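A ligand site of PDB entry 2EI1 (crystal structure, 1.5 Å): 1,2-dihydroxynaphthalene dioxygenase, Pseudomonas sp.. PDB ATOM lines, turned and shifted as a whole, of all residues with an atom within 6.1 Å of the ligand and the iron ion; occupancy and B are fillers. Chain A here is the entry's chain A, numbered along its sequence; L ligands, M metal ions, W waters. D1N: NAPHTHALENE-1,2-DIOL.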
ATOM      1  N   HIS A 152      10.955   9.935   9.367  1.00  0.00           N
ATOM      2  CA  HIS A 152      12.351   9.539   9.397  1.00  0.00           C
ATOM      3  C   HIS A 152      13.008   9.924  10.701  1.00  0.00           C
ATOM      4  O   HIS A 152      12.470  10.724  11.469  1.00  0.00           O
ATOM      5  CB  HIS A 152      13.147  10.116   8.203  1.00  0.00           C
ATOM      6  CG  HIS A 152      13.441  11.584   8.287  1.00  0.00           C
ATOM      7  ND1 HIS A 152      12.952  12.476   7.347  1.00  0.00           N
ATOM      8  CD2 HIS A 152      14.225  12.313   9.115  1.00  0.00           C
ATOM      9  CE1 HIS A 152      13.420  13.687   7.610  1.00  0.00           C
ATOM     10  NE2 HIS A 152      14.191  13.613   8.683  1.00  0.00           N
ATOM     11  N   CYS A 153      14.190   9.357  10.955  1.00  0.00           N
ATOM     12  CA  CYS A 153      14.993   9.800  12.099  1.00  0.00           C
ATOM     13  C   CYS A 153      16.472   9.887  11.763  1.00  0.00           C
ATOM     14  O   CYS A 153      16.949   9.175  10.880  1.00  0.00           O
ATOM     15  CB  CYS A 153      14.910   8.863  13.300  1.00  0.00           C
ATOM     16  SG  CYS A 153      13.355   8.291  13.963  1.00  0.00           S
ATOM     17  N   ILE A 154      17.182  10.727  12.524  1.00  0.00           N
ATOM     18  CA  ILE A 154      18.637  10.583  12.658  1.00  0.00           C
ATOM     19  C   ILE A 154      18.859   9.860  13.975  1.00  0.00           C
ATOM     20  O   ILE A 154      18.305  10.255  15.006  1.00  0.00           O
ATOM     21  CB  ILE A 154      19.400  11.929  12.631  1.00  0.00           C
ATOM     22  CG1 ILE A 154      19.432  12.489  11.189  1.00  0.00           C
ATOM     23  CG2 ILE A 154      20.832  11.775  13.198  1.00  0.00           C
ATOM     24  CD1 ILE A 154      20.282  13.755  11.037  1.00  0.00           C
ATOM     25  N   TYR A 178      25.483  15.390   2.609  1.00  0.00           N
ATOM     26  CA  TYR A 178      25.941  16.710   3.020  1.00  0.00           C
ATOM     27  C   TYR A 178      27.371  16.696   3.490  1.00  0.00           C
ATOM     28  O   TYR A 178      27.744  15.823   4.269  1.00  0.00           O
ATOM     29  CB  TYR A 178      25.100  17.263   4.161  1.00  0.00           C
ATOM     30  CG  TYR A 178      23.742  17.755   3.728  1.00  0.00           C
ATOM     31  CD1 TYR A 178      22.734  16.847   3.427  1.00  0.00           C
ATOM     32  CD2 TYR A 178      23.451  19.109   3.648  1.00  0.00           C
ATOM     33  CE1 TYR A 178      21.462  17.263   3.051  1.00  0.00           C
ATOM     34  CE2 TYR A 178      22.167  19.554   3.269  1.00  0.00           C
ATOM     35  CZ  TYR A 178      21.187  18.616   2.964  1.00  0.00           C
ATOM     36  OH  TYR A 178      19.891  18.977   2.616  1.00  0.00           O
ATOM     37  N   ILE A 180      29.239  19.565   5.252  1.00  0.00           N
ATOM     38  CA  ILE A 180      28.990  20.865   5.880  1.00  0.00           C
ATOM     39  C   ILE A 180      30.281  21.362   6.545  1.00  0.00           C
ATOM     40  O   ILE A 180      30.818  20.684   7.416  1.00  0.00           O
ATOM     41  CB  ILE A 180      27.906  20.755   6.982  1.00  0.00           C
ATOM     42  CG1 ILE A 180      26.593  20.227   6.395  1.00  0.00           C
ATOM     43  CG2 ILE A 180      27.720  22.109   7.690  1.00  0.00           C
ATOM     44  CD1 ILE A 180      25.729  19.481   7.411  1.00  0.00           C
ATOM     45  N   LEU A 190      27.095  13.814   6.495  1.00  0.00           N
ATOM     46  CA  LEU A 190      25.871  13.142   6.942  1.00  0.00           C
ATOM     47  C   LEU A 190      25.359  12.274   5.809  1.00  0.00           C
ATOM     48  O   LEU A 190      25.331  12.716   4.665  1.00  0.00           O
ATOM     49  CB  LEU A 190      24.804  14.160   7.362  1.00  0.00           C
ATOM     50  CG  LEU A 190      25.074  14.895   8.682  1.00  0.00           C
ATOM     51  CD1 LEU A 190      24.005  15.944   8.909  1.00  0.00           C
ATOM     52  CD2 LEU A 190      25.082  13.922   9.839  1.00  0.00           C
ATOM     53  N   PHE A 192      22.270   9.664   4.283  1.00  0.00           N
ATOM     54  CA  PHE A 192      20.795   9.577   4.295  1.00  0.00           C
ATOM     55  C   PHE A 192      20.377   8.402   3.451  1.00  0.00           C
ATOM     56  O   PHE A 192      20.777   8.314   2.272  1.00  0.00           O
ATOM     57  CB  PHE A 192      20.160  10.856   3.704  1.00  0.00           C
ATOM     58  CG  PHE A 192      20.478  12.094   4.489  1.00  0.00           C
ATOM     59  CD1 PHE A 192      21.743  12.692   4.406  1.00  0.00           C
ATOM     60  CD2 PHE A 192      19.512  12.686   5.314  1.00  0.00           C
ATOM     61  CE1 PHE A 192      22.056  13.838   5.132  1.00  0.00           C
ATOM     62  CE2 PHE A 192      19.829  13.825   6.062  1.00  0.00           C
ATOM     63  CZ  PHE A 192      21.086  14.402   5.978  1.00  0.00           C
ATOM     64  N   ASP A 199      11.983  10.658   0.945  1.00  0.00           N
ATOM     65  CA  ASP A 199      13.358  10.994   0.564  1.00  0.00           C
ATOM     66  C   ASP A 199      14.387  10.236   1.387  1.00  0.00           C
ATOM     67  O   ASP A 199      15.375   9.726   0.847  1.00  0.00           O
ATOM     68  CB  ASP A 199      13.638  12.478   0.656  1.00  0.00           C
ATOM     69  CG  ASP A 199      15.087  12.789   0.379  1.00  0.00           C
ATOM     70  OD1 ASP A 199      15.423  12.854  -0.824  1.00  0.00           O
ATOM     71  OD2 ASP A 199      15.851  12.891   1.355  1.00  0.00           O
ATOM     72  N   HIS A 200      14.168  10.142   2.693  1.00  0.00           N
ATOM     73  CA  HIS A 200      14.971   9.217   3.503  1.00  0.00           C
ATOM     74  C   HIS A 200      14.155   8.769   4.700  1.00  0.00           C
ATOM     75  O   HIS A 200      13.195   9.438   5.099  1.00  0.00           O
ATOM     76  CB  HIS A 200      16.318   9.796   3.911  1.00  0.00           C
ATOM     77  CG  HIS A 200      16.228  10.996   4.792  1.00  0.00           C
ATOM     78  ND1 HIS A 200      15.933  12.251   4.309  1.00  0.00           N
ATOM     79  CD2 HIS A 200      16.437  11.126   6.131  1.00  0.00           C
ATOM     80  CE1 HIS A 200      15.925  13.107   5.325  1.00  0.00           C
ATOM     81  NE2 HIS A 200      16.231  12.445   6.431  1.00  0.00           N
ATOM     82  N   ASN A 214      18.428  11.543  17.654  1.00  0.00           N
ATOM     83  CA  ASN A 214      18.669  12.967  17.436  1.00  0.00           C
ATOM     84  C   ASN A 214      17.363  13.699  17.137  1.00  0.00           C
ATOM     85  O   ASN A 214      17.019  14.674  17.810  1.00  0.00           O
ATOM     86  CB  ASN A 214      19.667  13.211  16.306  1.00  0.00           C
ATOM     87  CG  ASN A 214      19.800  14.685  15.979  1.00  0.00           C
ATOM     88  OD1 ASN A 214      19.194  15.181  15.011  1.00  0.00           O
ATOM     89  ND2 ASN A 214      20.570  15.415  16.803  1.00  0.00           N
ATOM     90  N   HIS A 215      16.638  13.239  16.118  1.00  0.00           N
ATOM     91  CA  HIS A 215      15.322  13.795  15.852  1.00  0.00           C
ATOM     92  C   HIS A 215      14.453  12.811  15.120  1.00  0.00           C
ATOM     93  O   HIS A 215      14.962  11.888  14.473  1.00  0.00           O
ATOM     94  CB  HIS A 215      15.393  15.122  15.062  1.00  0.00           C
ATOM     95  CG  HIS A 215      15.741  14.984  13.613  1.00  0.00           C
ATOM     96  ND1 HIS A 215      17.046  14.905  13.173  1.00  0.00           N
ATOM     97  CD2 HIS A 215      14.970  14.944  12.493  1.00  0.00           C
ATOM     98  CE1 HIS A 215      17.058  14.809  11.859  1.00  0.00           C
ATOM     99  NE2 HIS A 215      15.814  14.852  11.409  1.00  0.00           N
ATOM    100  N   MET A 217      11.261  13.136  12.310  1.00  0.00           N
ATOM    101  CA  MET A 217      10.543  14.025  11.403  1.00  0.00           C
ATOM    102  C   MET A 217       9.168  13.443  11.122  1.00  0.00           C
ATOM    103  O   MET A 217       9.063  12.260  10.766  1.00  0.00           O
ATOM    104  CB  MET A 217      11.339  14.146  10.101  1.00  0.00           C
ATOM    105  CG  MET A 217      10.823  15.196   9.131  1.00  0.00           C
ATOM    106  SD  MET A 217       9.493  14.596   8.057  1.00  0.00           S
ATOM    107  CE  MET A 217       9.198  16.105   7.130  1.00  0.00           C
ATOM    108  N   LEU A 242      16.481  24.634  15.353  1.00  0.00           N
ATOM    109  CA  LEU A 242      16.770  25.127  14.016  1.00  0.00           C
ATOM    110  C   LEU A 242      15.484  25.725  13.460  1.00  0.00           C
ATOM    111  O   LEU A 242      14.419  25.097  13.536  1.00  0.00           O
ATOM    112  CB  LEU A 242      17.290  24.020  13.092  1.00  0.00           C
ATOM    113  CG  LEU A 242      18.610  23.316  13.404  1.00  0.00           C
ATOM    114  CD1 LEU A 242      18.886  22.213  12.399  1.00  0.00           C
ATOM    115  CD2 LEU A 242      19.761  24.307  13.402  1.00  0.00           C
ATOM    116  N   HIS A 247      15.264  21.925   3.066  1.00  0.00           N
ATOM    117  CA  HIS A 247      16.405  21.062   2.876  1.00  0.00           C
ATOM    118  C   HIS A 247      16.726  20.897   1.403  1.00  0.00           C
ATOM    119  O   HIS A 247      15.826  20.730   0.570  1.00  0.00           O
ATOM    120  CB  HIS A 247      16.139  19.659   3.423  1.00  0.00           C
ATOM    121  CG  HIS A 247      16.057  19.579   4.903  1.00  0.00           C
ATOM    122  ND1 HIS A 247      17.086  19.964   5.751  1.00  0.00           N
ATOM    123  CD2 HIS A 247      15.088  19.065   5.701  1.00  0.00           C
ATOM    124  CE1 HIS A 247      16.729  19.716   6.998  1.00  0.00           C
ATOM    125  NE2 HIS A 247      15.518  19.177   6.996  1.00  0.00           N
ATOM    126  N   ALA A 248      18.025  20.863   1.102  1.00  0.00           N
ATOM    127  CA  ALA A 248      18.455  20.621  -0.279  1.00  0.00           C
ATOM    128  C   ALA A 248      18.150  19.216  -0.783  1.00  0.00           C
ATOM    129  O   ALA A 248      17.863  19.046  -1.971  1.00  0.00           O
ATOM    130  CB  ALA A 248      19.939  20.931  -0.418  1.00  0.00           C
ATOM    131  N   ASN A 249      18.187  18.223   0.106  1.00  0.00           N
ATOM    132  CA  ASN A 249      17.871  16.869  -0.351  1.00  0.00           C
ATOM    133  C   ASN A 249      16.384  16.609  -0.599  1.00  0.00           C
ATOM    134  O   ASN A 249      15.990  16.291  -1.730  1.00  0.00           O
ATOM    135  CB  ASN A 249      18.545  15.763   0.505  1.00  0.00           C
ATOM    136  CG  ASN A 249      18.215  15.830   1.990  1.00  0.00           C
ATOM    137  OD1 ASN A 249      17.422  16.664   2.451  1.00  0.00           O
ATOM    138  ND2 ASN A 249      18.812  14.919   2.746  1.00  0.00           N
ATOM    139  N   ASP A 250      15.549  16.804   0.433  1.00  0.00           N
ATOM    140  CA  ASP A 250      14.137  16.427   0.292  1.00  0.00           C
ATOM    141  C   ASP A 250      13.203  17.583  -0.071  1.00  0.00           C
ATOM    142  O   ASP A 250      12.025  17.363  -0.300  1.00  0.00           O
ATOM    143  CB  ASP A 250      13.631  15.665   1.519  1.00  0.00           C
ATOM    144  CG  ASP A 250      13.424  16.547   2.746  1.00  0.00           C
ATOM    145  OD1 ASP A 250      13.705  17.760   2.714  1.00  0.00           O
ATOM    146  OD2 ASP A 250      12.962  15.998   3.761  1.00  0.00           O
ATOM    147  N   THR A 254      10.658  22.692   6.893  1.00  0.00           N
ATOM    148  CA  THR A 254      10.656  22.086   8.230  1.00  0.00           C
ATOM    149  C   THR A 254      11.283  23.022   9.268  1.00  0.00           C
ATOM    150  O   THR A 254      11.987  23.969   8.909  1.00  0.00           O
ATOM    151  CB  THR A 254      11.451  20.736   8.302  1.00  0.00           C
ATOM    152  OG1 THR A 254      12.846  21.003   8.505  1.00  0.00           O
ATOM    153  CG2 THR A 254      11.262  19.834   7.072  1.00  0.00           C
ATOM    154  N   TYR A 256      12.902  22.534  13.669  1.00  0.00           N
ATOM    155  CA  TYR A 256      13.195  21.531  14.702  1.00  0.00           C
ATOM    156  C   TYR A 256      12.903  22.124  16.055  1.00  0.00           C
ATOM    157  O   TYR A 256      13.479  23.165  16.412  1.00  0.00           O
ATOM    158  CB  TYR A 256      14.649  21.079  14.663  1.00  0.00           C
ATOM    159  CG  TYR A 256      15.153  20.464  13.366  1.00  0.00           C
ATOM    160  CD1 TYR A 256      15.295  21.233  12.210  1.00  0.00           C
ATOM    161  CD2 TYR A 256      15.545  19.121  13.320  1.00  0.00           C
ATOM    162  CE1 TYR A 256      15.798  20.677  11.032  1.00  0.00           C
ATOM    163  CE2 TYR A 256      16.044  18.566  12.163  1.00  0.00           C
ATOM    164  CZ  TYR A 256      16.176  19.343  11.025  1.00  0.00           C
ATOM    165  OH  TYR A 256      16.688  18.772   9.870  1.00  0.00           O
ATOM    166  N   GLU A 266      10.998  17.199  14.219  1.00  0.00           N
ATOM    167  CA  GLU A 266      11.138  18.010  13.010  1.00  0.00           C
ATOM    168  C   GLU A 266       9.793  17.970  12.271  1.00  0.00           C
ATOM    169  O   GLU A 266       9.583  17.126  11.401  1.00  0.00           O
ATOM    170  CB  GLU A 266      12.262  17.447  12.108  1.00  0.00           C
ATOM    171  CG  GLU A 266      12.504  18.299  10.865  1.00  0.00           C
ATOM    172  CD  GLU A 266      13.493  17.688   9.891  1.00  0.00           C
ATOM    173  OE1 GLU A 266      13.882  16.513  10.063  1.00  0.00           O
ATOM    174  OE2 GLU A 266      13.838  18.396   8.912  1.00  0.00           O
ATOM    175  N   ASP A 284      21.816  24.106   2.918  1.00  0.00           N
ATOM    176  CA  ASP A 284      20.393  24.031   2.583  1.00  0.00           C
ATOM    177  C   ASP A 284      19.942  25.168   1.651  1.00  0.00           C
ATOM    178  O   ASP A 284      20.725  26.067   1.317  1.00  0.00           O
ATOM    179  CB  ASP A 284      19.558  23.912   3.868  1.00  0.00           C
ATOM    180  CG  ASP A 284      19.281  22.458   4.242  1.00  0.00           C
ATOM    181  OD1 ASP A 284      19.563  21.549   3.415  1.00  0.00           O
ATOM    182  OD2 ASP A 284      18.753  22.199   5.349  1.00  0.00           O
ATOM    183  N   LEU A 297      22.520  19.440  16.951  1.00  0.00           N
ATOM    184  CA  LEU A 297      22.448  19.866  15.557  1.00  0.00           C
ATOM    185  C   LEU A 297      22.941  21.301  15.381  1.00  0.00           C
ATOM    186  O   LEU A 297      22.234  22.146  14.862  1.00  0.00           O
ATOM    187  CB  LEU A 297      21.017  19.753  15.039  1.00  0.00           C
ATOM    188  CG  LEU A 297      20.554  18.415  14.477  1.00  0.00           C
ATOM    189  CD1 LEU A 297      19.174  18.565  13.858  1.00  0.00           C
ATOM    190  CD2 LEU A 297      21.504  17.856  13.455  1.00  0.00           C
ATOM    191  N   VAL A 299      24.877  22.661  13.256  1.00  0.00           N
ATOM    192  CA  VAL A 299      25.530  22.701  11.953  1.00  0.00           C
ATOM    193  C   VAL A 299      25.162  24.000  11.243  1.00  0.00           C
ATOM    194  O   VAL A 299      24.103  24.574  11.506  1.00  0.00           O
ATOM    195  CB  VAL A 299      25.072  21.535  11.052  1.00  0.00           C
ATOM    196  CG1 VAL A 299      25.737  20.236  11.456  1.00  0.00           C
ATOM    197  CG2 VAL A 299      23.578  21.393  11.072  1.00  0.00           C
ATOM    198  N   LEU A 301      23.864  25.549   8.039  1.00  0.00           N
ATOM    199  CA  LEU A 301      23.118  25.074   6.886  1.00  0.00           C
ATOM    200  C   LEU A 301      22.774  26.239   5.971  1.00  0.00           C
ATOM    201  O   LEU A 301      22.335  26.046   4.860  1.00  0.00           O
ATOM    202  CB  LEU A 301      21.852  24.399   7.367  1.00  0.00           C
ATOM    203  CG  LEU A 301      21.667  22.887   7.342  1.00  0.00           C
ATOM    204  CD1 LEU A 301      22.752  22.070   6.695  1.00  0.00           C
ATOM    205  CD2 LEU A 301      21.098  22.273   8.585  1.00  0.00           C
HETATM  206  O2  D1N L   1      15.667  15.758   7.239  1.00  0.00           O
HETATM  207  C2  D1N L   1      16.955  16.323   7.009  1.00  0.00           C
HETATM  208  C3  D1N L   1      17.422  16.604   5.718  1.00  0.00           C
HETATM  209  C4  D1N L   1      18.687  17.180   5.586  1.00  0.00           C
HETATM  210  C5  D1N L   1      19.487  17.445   6.714  1.00  0.00           C
HETATM  211  C10 D1N L   1      19.013  17.143   7.993  1.00  0.00           C
HETATM  212  C1  D1N L   1      17.743  16.589   8.125  1.00  0.00           C
HETATM  213  O1  D1N L   1      17.175  16.273   9.399  1.00  0.00           O
HETATM  214  C9  D1N L   1      19.788  17.417   9.148  1.00  0.00           C
HETATM  215  C8  D1N L   1      21.053  17.985   8.965  1.00  0.00           C
HETATM  216  C7  D1N L   1      21.528  18.273   7.675  1.00  0.00           C
HETATM  217  C6  D1N L   1      20.747  18.013   6.560  1.00  0.00           C
HETATM  218 FE    FE M   1      15.413  15.291   9.321  1.00  0.00          FE
HETATM  219  O   HOH W   1      13.017  16.667   6.376  1.00  0.00           O
HETATM  220  O   HOH W   2      17.124  13.578   8.836  1.00  0.00           O
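NE2 of His 247 lies close to O2 of the ligand, at 3.4 Å. A ring nitrogen (NE2) of His 200 lies close to an oxygen (O2) of the ligand. The side-chain hydroxyl (OH) of Tyr 256 sits close to an oxygen (O1) of the ligand, at 2.6 Å.
The backbone carbonyl oxygen (O) of His 152 sits at hydrogen-bond distance from the backbone NH (N) of Met 217 (2.8 Å). A ring nitrogen (ND1) of His 152 sits close to a ring nitrogen (NE2) of His 200, at 3.4 Å. A ring nitrogen (ND1) of His 247 lies within hydrogen-bond range of the side-chain carboxylate of Asp 284. N of Leu 190 sits at hydrogen-bond distance from O of Tyr 178 (3.1 Å). The side-chain carboxylate (OD2) of Asp 199 is in hydrogen-bond range of a ring nitrogen (ND1) of His 200, at 3.0 Å. The side-chain hydroxyl (OH) of Tyr 256 lies close to a ring nitrogen (NE2) of His 247 (3.1 Å). The side-chain carboxylate (OE2) of Glu 266 lies within hydrogen-bond range of the side-chain hydroxyl (OG1) of Thr 254 (2.8 Å). ND1 of His 215 lies within hydrogen-bond range of OD1 of Asn 214 (2.8 Å).
Residues that only touch the ligand: Asn 249 (3.3 Å), Phe 192 (3.5 Å), Leu 190 (3.6 Å) and Tyr 178 (3.7 Å). Hydrophobic or aromatic side chains that line the ligand: His 152, Tyr 178, Leu 190, Phe 192, His 200, His 215, His 247 and Tyr 256. Within 4 Å of the ligand: His 152, Tyr 178, Leu 190, Phe 192, His 200, His 215, His 247, Asn 249, Tyr 256 and Glu 266. The nearest printed residue that does not touch the ligand is Leu 301 (4.1 Å).
OH of Tyr 256 touches the iron ion (3.7 Å). Four residues have an atom within 4 Å of the iron ion: His 152, His 215, Tyr 256 and Glu 266.
The iron ion is bound by O1 of the ligand (2.0 Å), OE1 of Glu 266 (2.1 Å), O2 of the ligand (2.1 Å), NE2 of His 215 (2.2 Å), NE2 of His 152 (2.2 Å) and water W2 (2.5 Å).
Water W1 bridges the side-chain carboxylate (OD2) of Asp 250 (2.7 Å) and the side-chain carboxylate (OE2) of Glu 266 (3.2 Å).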
